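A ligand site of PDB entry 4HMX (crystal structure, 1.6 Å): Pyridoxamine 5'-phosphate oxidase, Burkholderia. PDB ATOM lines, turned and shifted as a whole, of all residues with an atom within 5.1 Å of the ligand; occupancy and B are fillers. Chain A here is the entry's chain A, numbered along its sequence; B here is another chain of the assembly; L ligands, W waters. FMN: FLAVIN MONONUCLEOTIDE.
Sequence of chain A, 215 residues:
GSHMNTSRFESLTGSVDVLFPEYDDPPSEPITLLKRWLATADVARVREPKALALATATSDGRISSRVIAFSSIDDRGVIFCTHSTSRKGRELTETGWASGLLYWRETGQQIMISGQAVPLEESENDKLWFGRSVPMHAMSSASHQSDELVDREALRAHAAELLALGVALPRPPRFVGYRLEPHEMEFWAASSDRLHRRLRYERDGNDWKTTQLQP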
ATOM      1  N   GLU A  48      -5.953   4.862  27.995  1.00  0.00           N
ATOM      2  CA  GLU A  48      -4.803   5.747  28.086  1.00  0.00           C
ATOM      3  C   GLU A  48      -4.789   6.578  29.378  1.00  0.00           C
ATOM      4  O   GLU A  48      -4.779   7.812  29.364  1.00  0.00           O
ATOM      5  CB  GLU A  48      -4.721   6.659  26.846  1.00  0.00           C
ATOM      6  CG  GLU A  48      -4.559   5.914  25.583  1.00  0.00           C
ATOM      7  CD  GLU A  48      -4.477   6.846  24.381  1.00  0.00           C
ATOM      8  OE1 GLU A  48      -3.898   7.961  24.522  1.00  0.00           O
ATOM      9  OE2 GLU A  48      -4.995   6.473  23.348  1.00  0.00           O
ATOM     10  N   ALA A  51      -2.046   9.541  29.748  1.00  0.00           N
ATOM     11  CA  ALA A  51      -1.959  10.629  28.815  1.00  0.00           C
ATOM     12  C   ALA A  51      -2.158  11.936  29.588  1.00  0.00           C
ATOM     13  O   ALA A  51      -3.258  12.277  30.028  1.00  0.00           O
ATOM     14  CB  ALA A  51      -3.048  10.520  27.730  1.00  0.00           C
ATOM     15  N   SER A  65       0.612  23.811  25.632  1.00  0.00           N
ATOM     16  CA  SER A  65       0.196  22.536  26.136  1.00  0.00           C
ATOM     17  C   SER A  65       0.214  21.458  25.047  1.00  0.00           C
ATOM     18  O   SER A  65       0.093  21.736  23.857  1.00  0.00           O
ATOM     19  CB  SER A  65      -1.191  22.658  26.791  1.00  0.00           C
ATOM     20  OG  SER A  65      -1.470  21.476  27.533  1.00  0.00           O
ATOM     21  N   ARG A  66       0.427  20.244  25.480  1.00  0.00           N
ATOM     22  CA  ARG A  66       0.402  19.040  24.591  1.00  0.00           C
ATOM     23  C   ARG A  66       0.270  17.785  25.434  1.00  0.00           C
ATOM     24  O   ARG A  66       0.590  17.773  26.652  1.00  0.00           O
ATOM     25  CB  ARG A  66       1.672  18.926  23.700  1.00  0.00           C
ATOM     26  CG  ARG A  66       2.928  18.467  24.436  1.00  0.00           C
ATOM     27  CD  ARG A  66       3.376  19.484  25.544  1.00  0.00           C
ATOM     28  NE  ARG A  66       3.845  20.692  24.882  1.00  0.00           N
ATOM     29  CZ  ARG A  66       4.078  21.838  25.508  1.00  0.00           C
ATOM     30  NH1 ARG A  66       4.561  22.867  24.816  1.00  0.00           N
ATOM     31  NH2 ARG A  66       3.794  22.012  26.814  1.00  0.00           N
ATOM     32  N   VAL A  67      -0.201  16.709  24.823  1.00  0.00           N
ATOM     33  CA  VAL A  67      -0.259  15.423  25.513  1.00  0.00           C
ATOM     34  C   VAL A  67       1.135  14.795  25.597  1.00  0.00           C
ATOM     35  O   VAL A  67       1.881  14.784  24.617  1.00  0.00           O
ATOM     36  CB  VAL A  67      -1.217  14.456  24.812  1.00  0.00           C
ATOM     37  CG1 VAL A  67      -1.284  13.080  25.532  1.00  0.00           C
ATOM     38  CG2 VAL A  67      -2.621  15.081  24.748  1.00  0.00           C
ATOM     39  N   ILE A  68       1.398  14.228  26.752  1.00  0.00           N
ATOM     40  CA  ILE A  68       2.625  13.449  26.990  1.00  0.00           C
ATOM     41  C   ILE A  68       2.194  12.168  27.693  1.00  0.00           C
ATOM     42  O   ILE A  68       1.493  12.235  28.712  1.00  0.00           O
ATOM     43  CB  ILE A  68       3.562  14.220  27.969  1.00  0.00           C
ATOM     44  CG1 ILE A  68       4.018  15.480  27.271  1.00  0.00           C
ATOM     45  CG2 ILE A  68       4.728  13.342  28.390  1.00  0.00           C
ATOM     46  CD1 ILE A  68       4.973  15.241  26.158  1.00  0.00           C
ATOM     47  N   ALA A  69       2.567  11.008  27.163  1.00  0.00           N
ATOM     48  CA  ALA A  69       2.342   9.775  27.876  1.00  0.00           C
ATOM     49  C   ALA A  69       3.556   9.568  28.774  1.00  0.00           C
ATOM     50  O   ALA A  69       4.624   9.202  28.310  1.00  0.00           O
ATOM     51  CB  ALA A  69       2.158   8.604  26.884  1.00  0.00           C
ATOM     52  N   CYS A  81       9.807  11.814  28.614  1.00  0.00           N
ATOM     53  CA  CYS A  81      10.819  12.103  27.641  1.00  0.00           C
ATOM     54  C   CYS A  81      10.289  12.942  26.504  1.00  0.00           C
ATOM     55  O   CYS A  81       9.093  12.928  26.199  1.00  0.00           O
ATOM     56  CB  CYS A  81      11.478  10.825  27.133  1.00  0.00           C
ATOM     57  SG  CYS A  81      10.439   9.632  26.353  1.00  0.00           S
ATOM     58  N   THR A  82      11.213  13.655  25.883  1.00  0.00           N
ATOM     59  CA  THR A  82      10.889  14.509  24.757  1.00  0.00           C
ATOM     60  C   THR A  82      12.175  14.960  24.045  1.00  0.00           C
ATOM     61  O   THR A  82      13.286  14.535  24.403  1.00  0.00           O
ATOM     62  CB  THR A  82      10.056  15.724  25.249  1.00  0.00           C
ATOM     63  OG1 THR A  82       9.461  16.397  24.139  1.00  0.00           O
ATOM     64  CG2 THR A  82      10.873  16.749  26.046  1.00  0.00           C
ATOM     65  N   HIS A  83      12.053  15.775  23.027  1.00  0.00           N
ATOM     66  CA  HIS A  83      13.226  16.385  22.419  1.00  0.00           C
ATOM     67  C   HIS A  83      13.549  17.724  23.083  1.00  0.00           C
ATOM     68  O   HIS A  83      12.662  18.580  23.251  1.00  0.00           O
ATOM     69  CB  HIS A  83      13.036  16.621  20.906  1.00  0.00           C
ATOM     70  CG  HIS A  83      12.977  15.362  20.103  1.00  0.00           C
ATOM     71  ND1 HIS A  83      13.201  15.325  18.748  1.00  0.00           N
ATOM     72  CD2 HIS A  83      12.669  14.110  20.468  1.00  0.00           C
ATOM     73  CE1 HIS A  83      13.050  14.095  18.306  1.00  0.00           C
ATOM     74  NE2 HIS A  83      12.730  13.327  19.341  1.00  0.00           N
ATOM     75  N   SER A  86      12.568  20.731  21.054  1.00  0.00           N
ATOM     76  CA  SER A  86      11.162  20.948  20.792  1.00  0.00           C
ATOM     77  C   SER A  86      10.720  22.266  21.452  1.00  0.00           C
ATOM     78  O   SER A  86      11.458  22.864  22.222  1.00  0.00           O
ATOM     79  CB  SER A  86      10.277  19.800  21.375  1.00  0.00           C
ATOM     80  OG  SER A  86      10.321  19.766  22.773  1.00  0.00           O
ATOM     81  N   ARG A  87       9.505  22.704  21.153  1.00  0.00           N
ATOM     82  CA  ARG A  87       8.960  23.899  21.755  1.00  0.00           C
ATOM     83  C   ARG A  87       8.846  23.738  23.279  1.00  0.00           C
ATOM     84  O   ARG A  87       9.293  24.622  24.031  1.00  0.00           O
ATOM     85  CB  ARG A  87       7.612  24.194  21.102  1.00  0.00           C
ATOM     86  CG  ARG A  87       6.994  25.507  21.500  1.00  0.00           C
ATOM     87  CD  ARG A  87       5.858  25.326  22.468  1.00  0.00           C
ATOM     88  NE  ARG A  87       5.204  26.607  22.651  1.00  0.00           N
ATOM     89  CZ  ARG A  87       4.342  27.130  21.806  1.00  0.00           C
ATOM     90  NH1 ARG A  87       3.982  26.438  20.732  1.00  0.00           N
ATOM     91  NH2 ARG A  87       3.827  28.355  22.048  1.00  0.00           N
ATOM     92  N   LYS A  88       8.324  22.602  23.760  1.00  0.00           N
ATOM     93  CA  LYS A  88       8.226  22.373  25.203  1.00  0.00           C
ATOM     94  C   LYS A  88       9.646  22.316  25.815  1.00  0.00           C
ATOM     95  O   LYS A  88       9.914  22.779  26.929  1.00  0.00           O
ATOM     96  CB  LYS A  88       7.436  21.113  25.558  1.00  0.00           C
ATOM     97  CG  LYS A  88       8.256  19.809  25.643  1.00  0.00           C
ATOM     98  CD  LYS A  88       7.354  18.606  25.690  1.00  0.00           C
ATOM     99  CE  LYS A  88       6.632  18.303  24.379  1.00  0.00           C
ATOM    100  NZ  LYS A  88       7.592  18.281  23.255  1.00  0.00           N
ATOM    101  N   GLY A  89      10.575  21.727  25.081  1.00  0.00           N
ATOM    102  CA  GLY A  89      11.942  21.557  25.581  1.00  0.00           C
ATOM    103  C   GLY A  89      12.585  22.903  25.840  1.00  0.00           C
ATOM    104  O   GLY A  89      13.235  23.096  26.863  1.00  0.00           O
ATOM    105  N   ARG A 132      12.515   2.094  24.591  1.00  0.00           N
ATOM    106  CA  ARG A 132      11.519   2.298  23.546  1.00  0.00           C
ATOM    107  C   ARG A 132      11.738   1.333  22.351  1.00  0.00           C
ATOM    108  O   ARG A 132      12.762   0.665  22.241  1.00  0.00           O
ATOM    109  CB  ARG A 132      11.545   3.754  23.063  1.00  0.00           C
ATOM    110  CG  ARG A 132      11.379   4.806  24.154  1.00  0.00           C
ATOM    111  CD  ARG A 132      10.084   4.601  24.907  1.00  0.00           C
ATOM    112  NE  ARG A 132       8.930   4.887  24.034  1.00  0.00           N
ATOM    113  CZ  ARG A 132       8.249   6.042  24.041  1.00  0.00           C
ATOM    114  NH1 ARG A 132       7.240   6.232  23.210  1.00  0.00           N
ATOM    115  NH2 ARG A 132       8.556   6.989  24.912  1.00  0.00           N
ATOM    116  N   GLN A 145      11.737  17.357  16.447  1.00  0.00           N
ATOM    117  CA  GLN A 145      10.411  17.646  16.917  1.00  0.00           C
ATOM    118  C   GLN A 145      10.121  19.141  17.060  1.00  0.00           C
ATOM    119  O   GLN A 145      10.877  19.904  17.708  1.00  0.00           O
ATOM    120  CB  GLN A 145      10.208  16.953  18.269  1.00  0.00           C
ATOM    121  CG  GLN A 145       8.798  17.082  18.857  1.00  0.00           C
ATOM    122  CD  GLN A 145       8.727  16.327  20.178  1.00  0.00           C
ATOM    123  OE1 GLN A 145       9.336  16.754  21.179  1.00  0.00           O
ATOM    124  NE2 GLN A 145       8.016  15.176  20.172  1.00  0.00           N
ATOM    125  N   SER A 146       8.998  19.536  16.439  1.00  0.00           N
ATOM    126  CA  SER A 146       8.504  20.910  16.442  1.00  0.00           C
ATOM    127  C   SER A 146       9.181  21.909  15.538  1.00  0.00           C
ATOM    128  O   SER A 146       8.671  23.039  15.412  1.00  0.00           O
ATOM    129  CB  SER A 146       8.385  21.456  17.894  1.00  0.00           C
ATOM    130  OG  SER A 146       7.656  20.527  18.665  1.00  0.00           O
ATOM    131  N   TYR B 103      -8.043  16.596  23.801  1.00  0.00           N
ATOM    132  CA  TYR B 103      -7.435  15.379  23.320  1.00  0.00           C
ATOM    133  C   TYR B 103      -8.503  14.323  23.209  1.00  0.00           C
ATOM    134  O   TYR B 103      -9.147  14.027  24.202  1.00  0.00           O
ATOM    135  CB  TYR B 103      -6.276  14.864  24.222  1.00  0.00           C
ATOM    136  CG  TYR B 103      -5.756  13.492  23.823  1.00  0.00           C
ATOM    137  CD1 TYR B 103      -5.455  13.222  22.513  1.00  0.00           C
ATOM    138  CD2 TYR B 103      -5.579  12.483  24.764  1.00  0.00           C
ATOM    139  CE1 TYR B 103      -5.010  11.937  22.112  1.00  0.00           C
ATOM    140  CE2 TYR B 103      -5.116  11.224  24.415  1.00  0.00           C
ATOM    141  CZ  TYR B 103      -4.832  10.939  23.059  1.00  0.00           C
ATOM    142  OH  TYR B 103      -4.385   9.671  22.641  1.00  0.00           O
ATOM    143  N   GLN B 110      -5.398  16.029  18.904  1.00  0.00           N
ATOM    144  CA  GLN B 110      -5.311  17.027  19.936  1.00  0.00           C
ATOM    145  C   GLN B 110      -5.438  18.434  19.282  1.00  0.00           C
ATOM    146  O   GLN B 110      -5.065  18.634  18.138  1.00  0.00           O
ATOM    147  CB  GLN B 110      -4.058  16.897  20.853  1.00  0.00           C
ATOM    148  CG  GLN B 110      -2.876  16.750  20.247  1.00  0.00           C
ATOM    149  CD  GLN B 110      -1.662  16.609  21.188  1.00  0.00           C
ATOM    150  OE1 GLN B 110      -1.605  17.134  22.328  1.00  0.00           O
ATOM    151  NE2 GLN B 110      -0.644  15.937  20.650  1.00  0.00           N
ATOM    152  N   GLU B 186      -2.748  24.812  17.642  1.00  0.00           N
ATOM    153  CA  GLU B 186      -2.122  23.690  16.918  1.00  0.00           C
ATOM    154  C   GLU B 186      -3.161  22.589  16.812  1.00  0.00           C
ATOM    155  O   GLU B 186      -3.859  22.292  17.798  1.00  0.00           O
ATOM    156  CB  GLU B 186      -0.889  23.071  17.593  1.00  0.00           C
ATOM    157  CG  GLU B 186      -0.336  21.958  16.616  1.00  0.00           C
ATOM    158  CD  GLU B 186       0.764  20.998  17.146  1.00  0.00           C
ATOM    159  OE1 GLU B 186       1.441  21.366  18.159  1.00  0.00           O
ATOM    160  OE2 GLU B 186       0.889  19.888  16.567  1.00  0.00           O
ATOM    161  N   TRP B 188      -3.324  18.567  15.791  1.00  0.00           N
ATOM    162  CA  TRP B 188      -2.452  17.411  15.694  1.00  0.00           C
ATOM    163  C   TRP B 188      -3.340  16.163  15.460  1.00  0.00           C
ATOM    164  O   TRP B 188      -4.348  15.985  16.135  1.00  0.00           O
ATOM    165  CB  TRP B 188      -1.724  17.262  17.028  1.00  0.00           C
ATOM    166  CG  TRP B 188      -0.716  16.117  17.189  1.00  0.00           C
ATOM    167  CD1 TRP B 188       0.652  16.232  17.125  1.00  0.00           C
ATOM    168  CD2 TRP B 188      -0.987  14.733  17.481  1.00  0.00           C
ATOM    169  NE1 TRP B 188       1.238  15.052  17.374  1.00  0.00           N
ATOM    170  CE2 TRP B 188       0.286  14.103  17.624  1.00  0.00           C
ATOM    171  CE3 TRP B 188      -2.140  13.994  17.740  1.00  0.00           C
ATOM    172  CZ2 TRP B 188       0.410  12.737  17.948  1.00  0.00           C
ATOM    173  CZ3 TRP B 188      -2.003  12.639  18.041  1.00  0.00           C
ATOM    174  CH2 TRP B 188      -0.736  12.029  18.163  1.00  0.00           C
ATOM    175  N   ARG B 198       0.776  17.875  11.924  1.00  0.00           N
ATOM    176  CA  ARG B 198       0.832  18.992  12.880  1.00  0.00           C
ATOM    177  C   ARG B 198       0.717  20.289  12.102  1.00  0.00           C
ATOM    178  O   ARG B 198       1.537  20.630  11.255  1.00  0.00           O
ATOM    179  CB  ARG B 198       2.174  18.997  13.576  1.00  0.00           C
ATOM    180  CG  ARG B 198       2.442  17.733  14.396  1.00  0.00           C
ATOM    181  CD  ARG B 198       3.655  17.907  15.310  1.00  0.00           C
ATOM    182  NE  ARG B 198       3.429  18.953  16.304  1.00  0.00           N
ATOM    183  CZ  ARG B 198       4.361  19.442  17.104  1.00  0.00           C
ATOM    184  NH1 ARG B 198       5.626  19.052  17.010  1.00  0.00           N
ATOM    185  NH2 ARG B 198       3.993  20.359  17.994  1.00  0.00           N
ATOM    186  N   ARG B 200       0.208  24.299  12.733  1.00  0.00           N
ATOM    187  CA  ARG B 200       0.288  25.424  13.671  1.00  0.00           C
ATOM    188  C   ARG B 200      -0.236  26.724  13.028  1.00  0.00           C
ATOM    189  O   ARG B 200       0.149  27.062  11.928  1.00  0.00           O
ATOM    190  CB  ARG B 200       1.718  25.652  14.137  1.00  0.00           C
ATOM    191  CG  ARG B 200       1.906  26.897  15.024  1.00  0.00           C
ATOM    192  CD  ARG B 200       3.352  27.187  15.304  1.00  0.00           C
ATOM    193  NE  ARG B 200       3.950  26.263  16.238  1.00  0.00           N
ATOM    194  CZ  ARG B 200       5.286  26.117  16.382  1.00  0.00           C
ATOM    195  NH1 ARG B 200       6.114  26.868  15.600  1.00  0.00           N
ATOM    196  NH2 ARG B 200       5.799  25.245  17.289  1.00  0.00           N
ATOM    197  N   PRO B 215       7.037  15.900  13.854  1.00  0.00           N
ATOM    198  CA  PRO B 215       6.403  15.232  14.989  1.00  0.00           C
ATOM    199  C   PRO B 215       7.330  14.937  16.143  1.00  0.00           C
ATOM    200  O   PRO B 215       6.779  14.835  17.289  1.00  0.00           O
ATOM    201  CB  PRO B 215       5.961  13.882  14.398  1.00  0.00           C
ATOM    202  CG  PRO B 215       6.958  13.612  13.222  1.00  0.00           C
ATOM    203  CD  PRO B 215       7.175  15.016  12.668  1.00  0.00           C
ATOM    204  OXT PRO B 215       8.563  14.851  15.959  1.00  0.00           O
HETATM  205  N1  FMN L   1       5.653  13.922  22.720  1.00  0.00           N
HETATM  206  C2  FMN L   1       6.802  13.747  23.437  1.00  0.00           C
HETATM  207  O2  FMN L   1       7.783  14.416  23.177  1.00  0.00           O
HETATM  208  N3  FMN L   1       6.866  12.798  24.438  1.00  0.00           N
HETATM  209  C4  FMN L   1       5.839  11.955  24.724  1.00  0.00           C
HETATM  210  O4  FMN L   1       5.911  11.098  25.650  1.00  0.00           O
HETATM  211  C4A FMN L   1       4.660  12.117  23.990  1.00  0.00           C
HETATM  212  N5  FMN L   1       3.594  11.265  24.208  1.00  0.00           N
HETATM  213  C5A FMN L   1       2.409  11.524  23.503  1.00  0.00           C
HETATM  214  C6  FMN L   1       1.283  10.716  23.707  1.00  0.00           C
HETATM  215  C7  FMN L   1       0.093  10.947  23.067  1.00  0.00           C
HETATM  216  C7M FMN L   1      -1.079  10.037  23.371  1.00  0.00           C
HETATM  217  C8  FMN L   1       0.009  11.936  22.110  1.00  0.00           C
HETATM  218  C8M FMN L   1      -1.299  12.177  21.436  1.00  0.00           C
HETATM  219  C9  FMN L   1       1.089  12.754  21.864  1.00  0.00           C
HETATM  220  C9A FMN L   1       2.316  12.516  22.543  1.00  0.00           C
HETATM  221  N10 FMN L   1       3.427  13.282  22.271  1.00  0.00           N
HETATM  222  C10 FMN L   1       4.593  13.102  22.996  1.00  0.00           C
HETATM  223  C1' FMN L   1       3.438  14.373  21.254  1.00  0.00           C
HETATM  224  C2' FMN L   1       3.179  15.731  21.897  1.00  0.00           C
HETATM  225  O2' FMN L   1       1.778  15.800  22.230  1.00  0.00           O
HETATM  226  C3' FMN L   1       3.597  16.904  21.027  1.00  0.00           C
HETATM  227  O3' FMN L   1       2.938  16.847  19.749  1.00  0.00           O
HETATM  228  C4' FMN L   1       5.120  16.985  20.806  1.00  0.00           C
HETATM  229  O4' FMN L   1       5.763  16.536  22.018  1.00  0.00           O
HETATM  230  C5' FMN L   1       5.517  18.431  20.434  1.00  0.00           C
HETATM  231  O5' FMN L   1       5.136  19.307  21.470  1.00  0.00           O
HETATM  232  P   FMN L   1       5.704  20.789  21.494  1.00  0.00           P
HETATM  233  O1P FMN L   1       7.117  20.733  22.048  1.00  0.00           O
HETATM  234  O2P FMN L   1       5.765  21.306  20.079  1.00  0.00           O
HETATM  235  O3P FMN L   1       4.725  21.514  22.352  1.00  0.00           O
HETATM  236  O   HOH W   1       4.090  15.213  17.660  1.00  0.00           O
HETATM  237  O   HOH W   2       4.712  23.789  19.363  1.00  0.00           O
HETATM  238  O   HOH W   3       7.213  10.483  27.987  1.00  0.00           O
HETATM  239  O   HOH W   4       1.251  18.954  19.779  1.00  0.00           O
HETATM  240  O   HOH W   5       2.355  22.366  21.807  1.00  0.00           O
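The side-chain hydroxyl of Ser 146 lies within hydrogen-bond range of an oxygen (O2P) of the ligand (2.5 Å).
An oxygen (O2') of the ligand sits at hydrogen-bond distance from the backbone NH of Val 67 (3.4 Å).
The backbone carbonyl oxygen of Val 67 sits at hydrogen-bond distance from an oxygen (O2') of the ligand (2.6 Å).
An oxygen (O2) of the ligand is in hydrogen-bond range of the side-chain hydroxyl (OG1) of Thr 82 (2.8 Å).
The backbone NH (N) of Lys 88 is in hydrogen-bond range of an oxygen (O1P) of the ligand (2.8 Å).
O1P of the ligand is in salt-bridge range of NZ of Lys 88.
The guanidinium group of Arg 66 lies within salt-bridge range of an oxygen (O3P) of the ligand.
The backbone carbonyl oxygen (O) of Cys 81 lies within hydrogen-bond range of a nitrogen (N3) of the ligand, 2.8 Å away.
NH2 of Arg 198 of chain B lies within salt-bridge range of O2P of the ligand, 2.9 Å away.
O2' of the ligand sits at hydrogen-bond distance from NE2 of Gln 110 of chain B (2.9 Å).
The side-chain amide nitrogen (NE2) of Gln 145 lies within hydrogen-bond range of an oxygen (O2) of the ligand (3.1 Å).
The backbone NH (N) of Ala 69 is in hydrogen-bond range of a nitrogen (N5) of the ligand, at 3.1 Å.
The backbone NH (N) of Arg 87 lies within hydrogen-bond range of an oxygen (O1P) of the ligand.
The indole nitrogen (NE1) of Trp 188 of chain B lies within hydrogen-bond range of an oxygen (O3') of the ligand, 3.4 Å away.
O1P of the ligand sits close to OG of Ser 86 (3.4 Å).
Merely in contact with the ligand: Tyr 103 of chain B (3.4 Å), Ile 68 (3.5 Å) and Glu 48 (3.7 Å).
Within 4 Å of the ligand: Glu 48, Arg 66, Val 67, Ile 68, Ala 69, Cys 81, Thr 82, Ser 86, Arg 87, Lys 88, Gln 145, Ser 146, Tyr 103 of chain B, Gln 110 of chain B, Trp 188 of chain B and Arg 198 of chain B.
Along chain A the residues within 4 Å of the ligand span positions 48 to 146.
The side-chain hydroxyl (OG) of Ser 146 is in hydrogen-bond range of the guanidinium group (NH1) of Arg 198 of chain B (3.0 Å).
The side-chain hydroxyl (OG1) of Thr 82 is in hydrogen-bond range of the side-chain amino group (NZ) of Lys 88.
OG1 of Thr 82 sits at hydrogen-bond distance from OE1 of Gln 145, 3.0 Å away.
The side-chain amino group (NZ) of Lys 88 sits at hydrogen-bond distance from the side-chain amide oxygen (OE1) of Gln 145 (3.1 Å).
The side-chain hydroxyl (OG) of Ser 86 sits at hydrogen-bond distance from the side-chain amino group (NZ) of Lys 88, 3.1 Å away.
The side-chain sulfur of Cys 81 is in hydrogen-bond range of the guanidinium group of Arg 132.
The backbone carbonyl oxygen (O) of Gln 110 of chain B lies within hydrogen-bond range of the backbone NH (N) of Trp 188 of chain B (2.9 Å).
The backbone NH (N) of Gln 145 is in hydrogen-bond range of a ring nitrogen (ND1) of His 83 (3.4 Å).
Water W5 lies within hydrogen-bond range of an oxygen (O3P) of the ligand (2.6 Å) and the backbone carbonyl oxygen of Ser 65 (3.1 Å).
Water W4 lies within hydrogen-bond range of an oxygen (O3') of the ligand (2.7 Å) and the side-chain carboxylate of Glu 186 of chain B (2.9 Å).
Water W3 lies within hydrogen-bond range of O4 of the ligand (2.7 Å), O of Ala 69 (2.9 Å) and N of Cys 81 (3.0 Å).
Water W2 lies within hydrogen-bond range of the guanidinium group of Arg 200 of chain B (2.8 Å), an oxygen (O2P) of the ligand (2.8 Å) and the guanidinium group of Arg 87 (3.1 Å).
Water W1 lies within hydrogen-bond range of the chain-end carboxylate (O) of Pro 215 of chain B (2.7 Å), the indole nitrogen (NE1) of Trp 188 of chain B (2.9 Å) and an oxygen (O3') of the ligand (2.9 Å).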
